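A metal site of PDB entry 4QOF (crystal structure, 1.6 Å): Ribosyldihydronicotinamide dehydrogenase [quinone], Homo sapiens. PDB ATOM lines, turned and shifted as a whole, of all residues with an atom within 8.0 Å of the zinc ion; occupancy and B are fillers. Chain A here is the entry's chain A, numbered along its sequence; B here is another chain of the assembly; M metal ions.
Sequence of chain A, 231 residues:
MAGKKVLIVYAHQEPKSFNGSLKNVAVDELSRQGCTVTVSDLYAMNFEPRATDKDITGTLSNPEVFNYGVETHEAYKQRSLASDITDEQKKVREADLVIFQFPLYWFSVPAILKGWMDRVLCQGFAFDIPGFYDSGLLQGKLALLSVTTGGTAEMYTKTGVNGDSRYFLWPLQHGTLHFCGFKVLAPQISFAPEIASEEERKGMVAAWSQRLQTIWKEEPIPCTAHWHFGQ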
ATOM      1  N   TYR A 133      24.919  -5.695  -8.442  1.00  0.00           N
ATOM      2  CA  TYR A 133      25.234  -4.528  -9.270  1.00  0.00           C
ATOM      3  C   TYR A 133      26.670  -4.725  -9.831  1.00  0.00           C
ATOM      4  O   TYR A 133      26.909  -5.790 -10.395  1.00  0.00           O
ATOM      5  CB  TYR A 133      24.962  -3.167  -8.557  1.00  0.00           C
ATOM      6  CG  TYR A 133      23.470  -2.878  -8.462  1.00  0.00           C
ATOM      7  CD1 TYR A 133      22.684  -2.789  -9.604  1.00  0.00           C
ATOM      8  CD2 TYR A 133      22.846  -2.715  -7.224  1.00  0.00           C
ATOM      9  CE1 TYR A 133      21.308  -2.605  -9.526  1.00  0.00           C
ATOM     10  CE2 TYR A 133      21.479  -2.488  -7.131  1.00  0.00           C
ATOM     11  CZ  TYR A 133      20.709  -2.403  -8.285  1.00  0.00           C
ATOM     12  OH  TYR A 133      19.355  -2.177  -8.242  1.00  0.00           O
ATOM     13  N   ASP A 134      27.621  -3.779  -9.589  1.00  0.00           N
ATOM     14  CA  ASP A 134      28.985  -3.945 -10.136  1.00  0.00           C
ATOM     15  C   ASP A 134      29.714  -5.200  -9.593  1.00  0.00           C
ATOM     16  O   ASP A 134      30.641  -5.682 -10.243  1.00  0.00           O
ATOM     17  CB  ASP A 134      29.827  -2.679  -9.982  1.00  0.00           C
ATOM     18  CG  ASP A 134      29.264  -1.479 -10.742  1.00  0.00           C
ATOM     19  OD1 ASP A 134      28.421  -1.680 -11.653  1.00  0.00           O
ATOM     20  OD2 ASP A 134      29.668  -0.334 -10.419  1.00  0.00           O
ATOM     21  N   TRP A 170      14.238   0.570 -17.133  1.00  0.00           N
ATOM     22  CA  TRP A 170      14.804   0.560 -15.785  1.00  0.00           C
ATOM     23  C   TRP A 170      14.686  -0.793 -15.042  1.00  0.00           C
ATOM     24  O   TRP A 170      15.718  -1.312 -14.616  1.00  0.00           O
ATOM     25  CB  TRP A 170      14.172   1.701 -14.954  1.00  0.00           C
ATOM     26  CG  TRP A 170      14.636   1.795 -13.536  1.00  0.00           C
ATOM     27  CD1 TRP A 170      13.911   1.505 -12.423  1.00  0.00           C
ATOM     28  CD2 TRP A 170      15.906   2.269 -13.086  1.00  0.00           C
ATOM     29  NE1 TRP A 170      14.657   1.757 -11.287  1.00  0.00           N
ATOM     30  CE2 TRP A 170      15.889   2.235 -11.669  1.00  0.00           C
ATOM     31  CE3 TRP A 170      17.070   2.736 -13.735  1.00  0.00           C
ATOM     32  CZ2 TRP A 170      16.973   2.673 -10.900  1.00  0.00           C
ATOM     33  CZ3 TRP A 170      18.152   3.132 -12.972  1.00  0.00           C
ATOM     34  CH2 TRP A 170      18.102   3.109 -11.568  1.00  0.00           C
ATOM     35  N   LEU A 172      14.336  -3.769 -16.135  1.00  0.00           N
ATOM     36  CA  LEU A 172      15.031  -4.811 -16.898  1.00  0.00           C
ATOM     37  C   LEU A 172      16.532  -4.595 -16.902  1.00  0.00           C
ATOM     38  O   LEU A 172      17.291  -5.446 -16.427  1.00  0.00           O
ATOM     39  CB  LEU A 172      14.479  -4.858 -18.328  1.00  0.00           C
ATOM     40  CG  LEU A 172      12.965  -5.180 -18.458  1.00  0.00           C
ATOM     41  CD1 LEU A 172      12.490  -4.971 -19.899  1.00  0.00           C
ATOM     42  CD2 LEU A 172      12.676  -6.572 -17.959  1.00  0.00           C
ATOM     43  N   GLN A 173      16.956  -3.453 -17.417  1.00  0.00           N
ATOM     44  CA  GLN A 173      18.372  -3.126 -17.531  1.00  0.00           C
ATOM     45  C   GLN A 173      19.026  -2.968 -16.169  1.00  0.00           C
ATOM     46  O   GLN A 173      20.068  -3.583 -15.933  1.00  0.00           O
ATOM     47  CB  GLN A 173      18.568  -1.848 -18.366  1.00  0.00           C
ATOM     48  CG  GLN A 173      18.145  -2.034 -19.819  1.00  0.00           C
ATOM     49  CD  GLN A 173      18.572  -0.933 -20.782  1.00  0.00           C
ATOM     50  OE1 GLN A 173      18.770  -1.182 -21.979  1.00  0.00           O
ATOM     51  NE2 GLN A 173      18.705   0.296 -20.302  1.00  0.00           N
ATOM     52  N   HIS A 174      18.452  -2.140 -15.286  1.00  0.00           N
ATOM     53  CA  HIS A 174      19.043  -1.875 -13.988  1.00  0.00           C
ATOM     54  C   HIS A 174      18.658  -2.900 -12.927  1.00  0.00           C
ATOM     55  O   HIS A 174      19.548  -3.553 -12.359  1.00  0.00           O
ATOM     56  CB  HIS A 174      18.754  -0.442 -13.501  1.00  0.00           C
ATOM     57  CG  HIS A 174      19.440  -0.100 -12.237  1.00  0.00           C
ATOM     58  ND1 HIS A 174      20.766   0.289 -12.221  1.00  0.00           N
ATOM     59  CD2 HIS A 174      18.965  -0.087 -10.959  1.00  0.00           C
ATOM     60  CE1 HIS A 174      21.061   0.555 -10.957  1.00  0.00           C
ATOM     61  NE2 HIS A 174      20.003   0.340 -10.165  1.00  0.00           N
ATOM     62  N   GLY A 175      17.363  -3.034 -12.647  1.00  0.00           N
ATOM     63  CA  GLY A 175      16.842  -3.908 -11.609  1.00  0.00           C
ATOM     64  C   GLY A 175      17.186  -5.364 -11.802  1.00  0.00           C
ATOM     65  O   GLY A 175      17.302  -6.102 -10.813  1.00  0.00           O
ATOM     66  N   THR A 176      17.388  -5.790 -13.074  1.00  0.00           N
ATOM     67  CA  THR A 176      17.680  -7.204 -13.346  1.00  0.00           C
ATOM     68  C   THR A 176      19.104  -7.427 -13.832  1.00  0.00           C
ATOM     69  O   THR A 176      19.908  -8.058 -13.133  1.00  0.00           O
ATOM     70  CB  THR A 176      16.640  -7.798 -14.327  1.00  0.00           C
ATOM     71  OG1 THR A 176      15.309  -7.485 -13.913  1.00  0.00           O
ATOM     72  CG2 THR A 176      16.799  -9.317 -14.456  1.00  0.00           C
ATOM     73  N   LEU A 177      19.419  -6.932 -15.037  1.00  0.00           N
ATOM     74  CA  LEU A 177      20.693  -7.194 -15.706  1.00  0.00           C
ATOM     75  C   LEU A 177      21.888  -6.616 -14.951  1.00  0.00           C
ATOM     76  O   LEU A 177      22.770  -7.369 -14.547  1.00  0.00           O
ATOM     77  CB  LEU A 177      20.652  -6.767 -17.184  1.00  0.00           C
ATOM     78  CG  LEU A 177      19.549  -7.492 -18.023  1.00  0.00           C
ATOM     79  CD1 LEU A 177      19.397  -6.854 -19.410  1.00  0.00           C
ATOM     80  CD2 LEU A 177      19.795  -8.998 -18.094  1.00  0.00           C
ATOM     81  N   HIS A 178      21.869  -5.311 -14.692  1.00  0.00           N
ATOM     82  CA  HIS A 178      22.949  -4.662 -13.943  1.00  0.00           C
ATOM     83  C   HIS A 178      23.042  -5.268 -12.525  1.00  0.00           C
ATOM     84  O   HIS A 178      24.160  -5.536 -12.080  1.00  0.00           O
ATOM     85  CB  HIS A 178      22.720  -3.149 -13.886  1.00  0.00           C
ATOM     86  CG  HIS A 178      23.835  -2.344 -13.271  1.00  0.00           C
ATOM     87  ND1 HIS A 178      23.693  -0.981 -13.088  1.00  0.00           N
ATOM     88  CD2 HIS A 178      25.048  -2.729 -12.800  1.00  0.00           C
ATOM     89  CE1 HIS A 178      24.832  -0.568 -12.540  1.00  0.00           C
ATOM     90  NE2 HIS A 178      25.680  -1.582 -12.350  1.00  0.00           N
ATOM     91  N   PHE A 179      21.881  -5.548 -11.862  1.00  0.00           N
ATOM     92  CA  PHE A 179      21.897  -6.172 -10.522  1.00  0.00           C
ATOM     93  C   PHE A 179      22.742  -7.465 -10.517  1.00  0.00           C
ATOM     94  O   PHE A 179      23.436  -7.728  -9.540  1.00  0.00           O
ATOM     95  CB  PHE A 179      20.489  -6.454  -9.995  1.00  0.00           C
ATOM     96  CG  PHE A 179      20.441  -6.900  -8.559  1.00  0.00           C
ATOM     97  CD1 PHE A 179      20.327  -5.966  -7.528  1.00  0.00           C
ATOM     98  CD2 PHE A 179      20.469  -8.251  -8.228  1.00  0.00           C
ATOM     99  CE1 PHE A 179      20.287  -6.380  -6.191  1.00  0.00           C
ATOM    100  CE2 PHE A 179      20.422  -8.667  -6.899  1.00  0.00           C
ATOM    101  CZ  PHE A 179      20.339  -7.727  -5.881  1.00  0.00           C
ATOM    102  N   PHE A 182      25.817  -7.818 -15.161  1.00  0.00           N
ATOM    103  CA  PHE A 182      25.997  -7.606 -16.587  1.00  0.00           C
ATOM    104  C   PHE A 182      26.338  -6.152 -16.889  1.00  0.00           C
ATOM    105  O   PHE A 182      25.899  -5.237 -16.188  1.00  0.00           O
ATOM    106  CB  PHE A 182      24.688  -7.879 -17.348  1.00  0.00           C
ATOM    107  CG  PHE A 182      24.295  -9.303 -17.573  1.00  0.00           C
ATOM    108  CD1 PHE A 182      24.859 -10.046 -18.612  1.00  0.00           C
ATOM    109  CD2 PHE A 182      23.267  -9.887 -16.829  1.00  0.00           C
ATOM    110  CE1 PHE A 182      24.442 -11.361 -18.867  1.00  0.00           C
ATOM    111  CE2 PHE A 182      22.832 -11.194 -17.110  1.00  0.00           C
ATOM    112  CZ  PHE A 182      23.428 -11.924 -18.111  1.00  0.00           C
ATOM    113  N   VAL A 184      25.511  -3.538 -19.700  1.00  0.00           N
ATOM    114  CA  VAL A 184      24.349  -3.435 -20.567  1.00  0.00           C
ATOM    115  C   VAL A 184      24.686  -2.682 -21.857  1.00  0.00           C
ATOM    116  O   VAL A 184      25.026  -1.510 -21.807  1.00  0.00           O
ATOM    117  CB  VAL A 184      23.154  -2.794 -19.797  1.00  0.00           C
ATOM    118  CG1 VAL A 184      21.920  -2.639 -20.691  1.00  0.00           C
ATOM    119  CG2 VAL A 184      22.808  -3.612 -18.532  1.00  0.00           C
ATOM    120  N   ILE A 221      26.334   0.963 -21.850  1.00  0.00           N
ATOM    121  CA  ILE A 221      25.765   2.224 -21.390  1.00  0.00           C
ATOM    122  C   ILE A 221      26.120   2.411 -19.908  1.00  0.00           C
ATOM    123  O   ILE A 221      26.369   1.425 -19.203  1.00  0.00           O
ATOM    124  CB  ILE A 221      24.207   2.249 -21.599  1.00  0.00           C
ATOM    125  CG1 ILE A 221      23.475   1.210 -20.683  1.00  0.00           C
ATOM    126  CG2 ILE A 221      23.803   2.098 -23.072  1.00  0.00           C
ATOM    127  CD1 ILE A 221      21.958   1.440 -20.420  1.00  0.00           C
ATOM    128  N   PRO A 222      26.105   3.642 -19.388  1.00  0.00           N
ATOM    129  CA  PRO A 222      26.256   3.813 -17.933  1.00  0.00           C
ATOM    130  C   PRO A 222      24.857   3.515 -17.373  1.00  0.00           C
ATOM    131  O   PRO A 222      23.934   4.315 -17.545  1.00  0.00           O
ATOM    132  CB  PRO A 222      26.647   5.285 -17.776  1.00  0.00           C
ATOM    133  CG  PRO A 222      26.167   5.980 -19.023  1.00  0.00           C
ATOM    134  CD  PRO A 222      25.862   4.936 -20.079  1.00  0.00           C
ATOM    135  N   CYS A 223      24.673   2.318 -16.814  1.00  0.00           N
ATOM    136  CA  CYS A 223      23.355   1.872 -16.353  1.00  0.00           C
ATOM    137  C   CYS A 223      22.953   2.524 -15.011  1.00  0.00           C
ATOM    138  O   CYS A 223      22.988   1.912 -13.931  1.00  0.00           O
ATOM    139  CB  CYS A 223      23.265   0.345 -16.321  1.00  0.00           C
ATOM    140  SG  CYS A 223      21.586  -0.252 -16.032  1.00  0.00           S
ATOM    141  N   THR A 224      22.640   3.836 -15.083  1.00  0.00           N
ATOM    142  CA  THR A 224      22.322   4.652 -13.915  1.00  0.00           C
ATOM    143  C   THR A 224      20.946   5.301 -14.028  1.00  0.00           C
ATOM    144  O   THR A 224      20.374   5.356 -15.132  1.00  0.00           O
ATOM    145  CB  THR A 224      23.364   5.760 -13.802  1.00  0.00           C
ATOM    146  OG1 THR A 224      23.240   6.612 -14.952  1.00  0.00           O
ATOM    147  CG2 THR A 224      24.795   5.222 -13.667  1.00  0.00           C
ATOM    148  N   ALA A 225      20.450   5.871 -12.898  1.00  0.00           N
ATOM    149  CA  ALA A 225      19.190   6.609 -12.856  1.00  0.00           C
ATOM    150  C   ALA A 225      19.269   7.799 -13.846  1.00  0.00           C
ATOM    151  O   ALA A 225      18.329   8.014 -14.595  1.00  0.00           O
ATOM    152  CB  ALA A 225      18.918   7.108 -11.447  1.00  0.00           C
ATOM    153  N   TRP A 227      20.991   8.063 -16.704  1.00  0.00           N
ATOM    154  CA  TRP A 227      20.833   7.610 -18.083  1.00  0.00           C
ATOM    155  C   TRP A 227      19.363   7.338 -18.420  1.00  0.00           C
ATOM    156  O   TRP A 227      18.898   7.759 -19.482  1.00  0.00           O
ATOM    157  CB  TRP A 227      21.677   6.351 -18.339  1.00  0.00           C
ATOM    158  CG  TRP A 227      21.691   5.902 -19.779  1.00  0.00           C
ATOM    159  CD1 TRP A 227      22.594   6.265 -20.733  1.00  0.00           C
ATOM    160  CD2 TRP A 227      20.764   5.006 -20.405  1.00  0.00           C
ATOM    161  NE1 TRP A 227      22.293   5.635 -21.928  1.00  0.00           N
ATOM    162  CE2 TRP A 227      21.168   4.874 -21.754  1.00  0.00           C
ATOM    163  CE3 TRP A 227      19.604   4.326 -19.969  1.00  0.00           C
ATOM    164  CZ2 TRP A 227      20.453   4.059 -22.662  1.00  0.00           C
ATOM    165  CZ3 TRP A 227      18.911   3.531 -20.870  1.00  0.00           C
ATOM    166  CH2 TRP A 227      19.329   3.420 -22.208  1.00  0.00           C
ATOM    167  N   HIS A 228      18.637   6.687 -17.499  1.00  0.00           N
ATOM    168  CA  HIS A 228      17.241   6.336 -17.733  1.00  0.00           C
ATOM    169  C   HIS A 228      16.261   7.508 -17.628  1.00  0.00           C
ATOM    170  O   HIS A 228      15.313   7.576 -18.407  1.00  0.00           O
ATOM    171  CB  HIS A 228      16.806   5.192 -16.784  1.00  0.00           C
ATOM    172  CG  HIS A 228      17.459   3.881 -17.087  1.00  0.00           C
ATOM    173  ND1 HIS A 228      18.728   3.586 -16.605  1.00  0.00           N
ATOM    174  CD2 HIS A 228      16.971   2.787 -17.734  1.00  0.00           C
ATOM    175  CE1 HIS A 228      18.984   2.344 -17.009  1.00  0.00           C
ATOM    176  NE2 HIS A 228      17.978   1.831 -17.703  1.00  0.00           N
ATOM    177  N   VAL B 161      20.999   2.456  -4.021  1.00  0.00           N
ATOM    178  CA  VAL B 161      21.447   1.534  -5.089  1.00  0.00           C
ATOM    179  C   VAL B 161      20.324   1.116  -6.047  1.00  0.00           C
ATOM    180  O   VAL B 161      20.572   0.885  -7.235  1.00  0.00           O
ATOM    181  CB  VAL B 161      22.229   0.282  -4.562  1.00  0.00           C
ATOM    182  CG1 VAL B 161      23.575   0.695  -3.962  1.00  0.00           C
ATOM    183  CG2 VAL B 161      21.402  -0.528  -3.556  1.00  0.00           C
HETATM  184 ZN    ZN M   1      22.085   0.071 -13.741  1.00  0.00          ZN
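N of His 178 lies within hydrogen-bond range of O of Gln 173 (2.8 Å).
The backbone carbonyl oxygen (O) of Val 161 of chain B lies within hydrogen-bond range of a ring nitrogen (NE2) of His 174, 3.0 Å away.
The backbone carbonyl oxygen of His 174 sits at hydrogen-bond distance from the backbone NH of Phe 179 (3.1 Å).
SG of Cys 223 sits close to O of Gln 173 (3.7 Å).
OH of Tyr 133 is in hydrogen-bond range of NE2 of His 174, 3.2 Å away.
OD1 of Asp 134 is in hydrogen-bond range of NE2 of His 178.
Along chain A the residues within 4 Å of the zinc ion span positions 174 to 223.
The zinc ion is bound by ND1 of His 174, 2.0 Å away.
The zinc ion is bound by a ring nitrogen (ND1) of His 178, at 2.0 Å.
O of Cys 223 is bound to the zinc ion, 2.1 Å away.
SG of Cys 223 binds the zinc ion (2.4 Å).
The zinc ion has four donor atoms within binding distance.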
